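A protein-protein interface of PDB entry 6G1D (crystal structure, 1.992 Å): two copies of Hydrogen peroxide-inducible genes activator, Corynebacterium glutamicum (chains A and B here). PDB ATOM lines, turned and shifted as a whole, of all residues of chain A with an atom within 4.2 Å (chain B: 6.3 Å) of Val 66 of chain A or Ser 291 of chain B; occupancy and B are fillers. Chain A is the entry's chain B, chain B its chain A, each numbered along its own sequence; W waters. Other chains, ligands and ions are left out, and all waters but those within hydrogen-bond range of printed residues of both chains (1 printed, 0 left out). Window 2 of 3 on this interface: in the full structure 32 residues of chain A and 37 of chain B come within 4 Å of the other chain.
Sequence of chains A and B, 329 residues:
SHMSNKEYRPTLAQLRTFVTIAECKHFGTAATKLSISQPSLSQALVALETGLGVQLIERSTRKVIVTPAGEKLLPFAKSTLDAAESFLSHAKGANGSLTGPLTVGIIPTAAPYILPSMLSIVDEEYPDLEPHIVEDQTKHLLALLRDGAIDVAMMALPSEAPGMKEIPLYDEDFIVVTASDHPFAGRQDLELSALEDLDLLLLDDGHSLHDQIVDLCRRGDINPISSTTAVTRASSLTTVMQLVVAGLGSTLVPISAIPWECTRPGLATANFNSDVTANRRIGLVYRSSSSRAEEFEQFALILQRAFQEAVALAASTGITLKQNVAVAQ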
ATOM      1  N   ALA A  22     -25.161  15.387 -15.345  1.00  0.00           N
ATOM      2  CA  ALA A  22     -25.383  16.384 -16.422  1.00  0.00           C
ATOM      3  C   ALA A  22     -24.496  17.600 -16.240  1.00  0.00           C
ATOM      4  O   ALA A  22     -24.005  18.134 -17.223  1.00  0.00           O
ATOM      5  CB  ALA A  22     -26.847  16.814 -16.476  1.00  0.00           C
ATOM      6  N   LEU A  56     -31.247   9.220 -20.912  1.00  0.00           N
ATOM      7  CA  LEU A  56     -30.933  10.585 -20.496  1.00  0.00           C
ATOM      8  C   LEU A  56     -29.480  10.999 -20.722  1.00  0.00           C
ATOM      9  O   LEU A  56     -29.178  12.179 -20.864  1.00  0.00           O
ATOM     10  CB  LEU A  56     -31.258  10.756 -19.013  1.00  0.00           C
ATOM     11  CG  LEU A  56     -32.700  10.480 -18.596  1.00  0.00           C
ATOM     12  CD1 LEU A  56     -32.831  10.571 -17.087  1.00  0.00           C
ATOM     13  CD2 LEU A  56     -33.671  11.469 -19.238  1.00  0.00           C
ATOM     14  N   ILE A  57     -28.582  10.022 -20.740  1.00  0.00           N
ATOM     15  CA  ILE A  57     -27.144  10.235 -20.869  1.00  0.00           C
ATOM     16  C   ILE A  57     -26.577   9.200 -21.843  1.00  0.00           C
ATOM     17  O   ILE A  57     -26.882   8.032 -21.725  1.00  0.00           O
ATOM     18  CB  ILE A  57     -26.438  10.019 -19.509  1.00  0.00           C
ATOM     19  CG1 ILE A  57     -26.997  10.947 -18.411  1.00  0.00           C
ATOM     20  CG2 ILE A  57     -24.926  10.167 -19.646  1.00  0.00           C
ATOM     21  CD1 ILE A  57     -26.679  12.412 -18.557  1.00  0.00           C
ATOM     22  N   ILE A  65     -22.305  12.854 -22.111  1.00  0.00           N
ATOM     23  CA  ILE A  65     -23.084  13.894 -22.774  1.00  0.00           C
ATOM     24  C   ILE A  65     -24.582  13.583 -22.582  1.00  0.00           C
ATOM     25  O   ILE A  65     -25.001  12.411 -22.594  1.00  0.00           O
ATOM     26  CB  ILE A  65     -22.686  13.915 -24.273  1.00  0.00           C
ATOM     27  CG1 ILE A  65     -21.207  14.303 -24.413  1.00  0.00           C
ATOM     28  CG2 ILE A  65     -23.625  14.769 -25.135  1.00  0.00           C
ATOM     29  CD1 ILE A  65     -20.568  13.902 -25.732  1.00  0.00           C
ATOM     30  N   VAL A  66     -25.284  14.629 -22.174  1.00  0.00           N
ATOM     31  CA  VAL A  66     -26.775  14.539 -22.085  1.00  0.00           C
ATOM     32  C   VAL A  66     -27.528  14.408 -23.546  1.00  0.00           C
ATOM     33  O   VAL A  66     -27.197  14.927 -24.671  1.00  0.00           O
ATOM     34  CB  VAL A  66     -27.266  15.817 -21.344  1.00  0.00           C
ATOM     35  CG1 VAL A  66     -28.716  15.740 -20.973  1.00  0.00           C
ATOM     36  CG2 VAL A  66     -26.480  16.019 -20.038  1.00  0.00           C
ATOM     37  N   THR A  67     -28.426  13.457 -23.535  1.00  0.00           N
ATOM     38  CA  THR A  67     -29.208  13.260 -24.779  1.00  0.00           C
ATOM     39  C   THR A  67     -30.193  14.420 -24.983  1.00  0.00           C
ATOM     40  O   THR A  67     -30.451  15.182 -24.045  1.00  0.00           O
ATOM     41  CB  THR A  67     -30.027  11.956 -24.769  1.00  0.00           C
ATOM     42  OG1 THR A  67     -30.997  12.012 -23.728  1.00  0.00           O
ATOM     43  CG2 THR A  67     -29.150  10.733 -24.595  1.00  0.00           C
ATOM     44  N   PRO A  68     -30.780  14.535 -26.194  1.00  0.00           N
ATOM     45  CA  PRO A  68     -31.860  15.548 -26.360  1.00  0.00           C
ATOM     46  C   PRO A  68     -32.968  15.426 -25.306  1.00  0.00           C
ATOM     47  O   PRO A  68     -33.349  16.417 -24.699  1.00  0.00           O
ATOM     48  CB  PRO A  68     -32.378  15.281 -27.771  1.00  0.00           C
ATOM     49  CG  PRO A  68     -31.216  14.693 -28.500  1.00  0.00           C
ATOM     50  CD  PRO A  68     -30.325  13.995 -27.489  1.00  0.00           C
ATOM     51  N   GLY A  70     -32.671  14.063 -22.290  1.00  0.00           N
ATOM     52  CA  GLY A  70     -32.092  14.494 -20.994  1.00  0.00           C
ATOM     53  C   GLY A  70     -32.020  15.997 -20.859  1.00  0.00           C
ATOM     54  O   GLY A  70     -32.333  16.536 -19.821  1.00  0.00           O
ATOM     55  N   GLU A  71     -31.653  16.677 -21.932  1.00  0.00           N
ATOM     56  CA  GLU A  71     -31.608  18.148 -21.925  1.00  0.00           C
ATOM     57  C   GLU A  71     -32.998  18.751 -21.684  1.00  0.00           C
ATOM     58  O   GLU A  71     -33.134  19.721 -20.956  1.00  0.00           O
ATOM     59  CB  GLU A  71     -30.990  18.665 -23.220  1.00  0.00           C
ATOM     60  CG  GLU A  71     -30.752  20.172 -23.245  1.00  0.00           C
ATOM     61  CD  GLU A  71     -30.023  20.628 -24.515  1.00  0.00           C
ATOM     62  OE1 GLU A  71     -29.125  19.891 -25.005  1.00  0.00           O
ATOM     63  OE2 GLU A  71     -30.359  21.715 -25.060  1.00  0.00           O
ATOM     64  N   ARG B 287     -27.200  27.758 -28.150  1.00  0.00           N
ATOM     65  CA  ARG B 287     -25.906  27.373 -27.500  1.00  0.00           C
ATOM     66  C   ARG B 287     -25.289  26.171 -28.206  1.00  0.00           C
ATOM     67  O   ARG B 287     -25.960  25.160 -28.387  1.00  0.00           O
ATOM     68  CB  ARG B 287     -26.124  26.985 -26.058  1.00  0.00           C
ATOM     69  CG  ARG B 287     -26.551  28.090 -25.148  1.00  0.00           C
ATOM     70  CD  ARG B 287     -27.128  27.490 -23.859  1.00  0.00           C
ATOM     71  NE  ARG B 287     -26.303  27.759 -22.693  1.00  0.00           N
ATOM     72  CZ  ARG B 287     -26.609  27.384 -21.453  1.00  0.00           C
ATOM     73  NH1 ARG B 287     -27.704  26.644 -21.184  1.00  0.00           N
ATOM     74  NH2 ARG B 287     -25.782  27.683 -20.452  1.00  0.00           N
ATOM     75  N   SER B 288     -24.031  26.280 -28.609  1.00  0.00           N
ATOM     76  CA  SER B 288     -23.351  25.171 -29.304  1.00  0.00           C
ATOM     77  C   SER B 288     -23.161  23.940 -28.415  1.00  0.00           C
ATOM     78  O   SER B 288     -22.941  22.847 -28.903  1.00  0.00           O
ATOM     79  CB  SER B 288     -22.004  25.638 -29.901  1.00  0.00           C
ATOM     80  OG  SER B 288     -21.166  26.136 -28.898  1.00  0.00           O
ATOM     81  N   SER B 289     -23.264  24.112 -27.099  1.00  0.00           N
ATOM     82  CA  SER B 289     -23.273  22.991 -26.166  1.00  0.00           C
ATOM     83  C   SER B 289     -24.584  22.201 -26.179  1.00  0.00           C
ATOM     84  O   SER B 289     -24.639  21.104 -25.655  1.00  0.00           O
ATOM     85  CB  SER B 289     -23.013  23.495 -24.750  1.00  0.00           C
ATOM     86  OG  SER B 289     -24.010  24.422 -24.371  1.00  0.00           O
ATOM     87  N   SER B 290     -25.653  22.739 -26.764  1.00  0.00           N
ATOM     88  CA  SER B 290     -26.912  22.008 -26.837  1.00  0.00           C
ATOM     89  C   SER B 290     -26.765  20.705 -27.627  1.00  0.00           C
ATOM     90  O   SER B 290     -26.015  20.638 -28.579  1.00  0.00           O
ATOM     91  CB  SER B 290     -27.997  22.890 -27.437  1.00  0.00           C
ATOM     92  OG  SER B 290     -29.233  22.192 -27.504  1.00  0.00           O
ATOM     93  N   SER B 291     -27.509  19.684 -27.229  1.00  0.00           N
ATOM     94  CA  SER B 291     -27.592  18.447 -28.001  1.00  0.00           C
ATOM     95  C   SER B 291     -28.814  18.452 -28.951  1.00  0.00           C
ATOM     96  O   SER B 291     -29.077  17.454 -29.620  1.00  0.00           O
ATOM     97  CB  SER B 291     -27.689  17.277 -27.044  1.00  0.00           C
ATOM     98  OG  SER B 291     -28.817  17.462 -26.196  1.00  0.00           O
ATOM     99  N   ARG B 292     -29.558  19.563 -28.992  1.00  0.00           N
ATOM    100  CA  ARG B 292     -30.852  19.587 -29.667  1.00  0.00           C
ATOM    101  C   ARG B 292     -30.834  20.150 -31.100  1.00  0.00           C
ATOM    102  O   ARG B 292     -31.871  20.609 -31.608  1.00  0.00           O
ATOM    103  CB  ARG B 292     -31.875  20.330 -28.799  1.00  0.00           C
ATOM    104  CG  ARG B 292     -32.099  19.662 -27.453  1.00  0.00           C
ATOM    105  CD  ARG B 292     -33.047  20.477 -26.614  1.00  0.00           C
ATOM    106  NE  ARG B 292     -34.400  20.378 -27.106  1.00  0.00           N
ATOM    107  CZ  ARG B 292     -35.437  21.078 -26.654  1.00  0.00           C
ATOM    108  NH1 ARG B 292     -35.292  21.960 -25.677  1.00  0.00           N
ATOM    109  NH2 ARG B 292     -36.648  20.860 -27.174  1.00  0.00           N
ATOM    110  N   ALA B 293     -29.691  20.054 -31.768  1.00  0.00           N
ATOM    111  CA  ALA B 293     -29.555  20.484 -33.153  1.00  0.00           C
ATOM    112  C   ALA B 293     -30.721  20.065 -34.036  1.00  0.00           C
ATOM    113  O   ALA B 293     -31.272  20.882 -34.794  1.00  0.00           O
ATOM    114  CB  ALA B 293     -28.250  19.989 -33.755  1.00  0.00           C
ATOM    115  N   GLU B 294     -31.095  18.792 -33.955  1.00  0.00           N
ATOM    116  CA  GLU B 294     -32.103  18.226 -34.848  1.00  0.00           C
ATOM    117  C   GLU B 294     -33.464  18.893 -34.639  1.00  0.00           C
ATOM    118  O   GLU B 294     -34.117  19.233 -35.606  1.00  0.00           O
ATOM    119  CB  GLU B 294     -32.208  16.723 -34.665  1.00  0.00           C
ATOM    120  CG  GLU B 294     -32.860  15.949 -35.795  1.00  0.00           C
ATOM    121  CD  GLU B 294     -32.744  14.427 -35.593  1.00  0.00           C
ATOM    122  OE1 GLU B 294     -31.703  13.939 -35.051  1.00  0.00           O
ATOM    123  OE2 GLU B 294     -33.704  13.708 -35.974  1.00  0.00           O
ATOM    124  N   GLU B 295     -33.873  19.083 -33.384  1.00  0.00           N
ATOM    125  CA  GLU B 295     -35.087  19.822 -33.074  1.00  0.00           C
ATOM    126  C   GLU B 295     -35.052  21.288 -33.478  1.00  0.00           C
ATOM    127  O   GLU B 295     -36.011  21.821 -33.948  1.00  0.00           O
ATOM    128  CB  GLU B 295     -35.387  19.760 -31.580  1.00  0.00           C
ATOM    129  CG  GLU B 295     -35.996  18.439 -31.148  1.00  0.00           C
ATOM    130  CD  GLU B 295     -36.048  18.359 -29.630  1.00  0.00           C
ATOM    131  OE1 GLU B 295     -35.005  18.110 -28.994  1.00  0.00           O
ATOM    132  OE2 GLU B 295     -37.132  18.607 -29.070  1.00  0.00           O
HETATM  133  O   HOH W   1     -32.808  22.932 -24.558  1.00  0.00           O
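O of Val 66 of chain A is in hydrogen-bond range of OG of Ser 291 of chain B (3.4 Å). OE2 of Glu 71 of chain A lies within hydrogen-bond range of OG of Ser 290 of chain B (2.7 Å). The side-chain carboxylate (OE1) of Glu 71 of chain A is in hydrogen-bond range of the side-chain hydroxyl (OG) of Ser 291 of chain B.
O of Leu 56 of chain A lies within hydrogen-bond range of N of Thr 67 of chain A (3.1 Å). The backbone NH (N) of Gly 70 of chain A is in hydrogen-bond range of the side-chain hydroxyl (OG1) of Thr 67 of chain A (3.0 Å). OG of Ser 290 of chain B lies within hydrogen-bond range of N of Arg 292 of chain B, 3.0 Å away. OE2 of Glu 295 of chain B lies within salt-bridge range of NH2 of Arg 292 of chain B (3.0 Å).
Among the printed residues, pairs that only touch across the chains: Glu 71 of chain A with Arg 292 of chain B (3.3 Å), Pro 68 of chain A with Ser 291 of chain B (3.5 Å) and Thr 67 of chain A with Ser 291 of chain B (3.5 Å).
Ile 57 of chain A touches none of the printed residues of chain B. Of the printed residues of chain B, Val 66 of chain A touches Ser 291 (3.4 Å). Printed residues of chain B within 4 Å of Thr 67 of chain A: Ser 291 (3.5 Å). Of the printed residues of chain B, Pro 68 of chain A touches Ser 291 (3.5 Å). Of the printed residues of chain B, Glu 71 of chain A touches Ser 290, Ser 291 and Arg 292. Ser 288 of chain B touches none of the printed residues of chain A. Printed residues of chain A within 4 Å of Ser 291 of chain B: Val 66 (3.4 Å), Thr 67 (3.5 Å), Pro 68 (3.5 Å) and Glu 71 (2.7 Å). The nearest printed residue of chain A that does not touch Ser 291 of chain B is Ile 65 of chain A (5.1 Å). The nearest printed residue of chain A that does not touch Arg 292 of chain B is Pro 68 of chain A (4.3 Å).
Hydrophobic or aromatic side chains of chain A that line the printed part of chain B: Pro 68. Along chain A the printed residues that touch a printed residue of chain B span positions 66 to 71. Among the printed residues, no Asp or Glu carboxylate lies within 4 Å of a Lys or Arg side-chain nitrogen of the other chain.
No position is printed for both chains.
Water W1 bridges OE2 of Glu 71 of chain A (2.8 Å) and NH1 of Arg 292 of chain B (2.9 Å).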
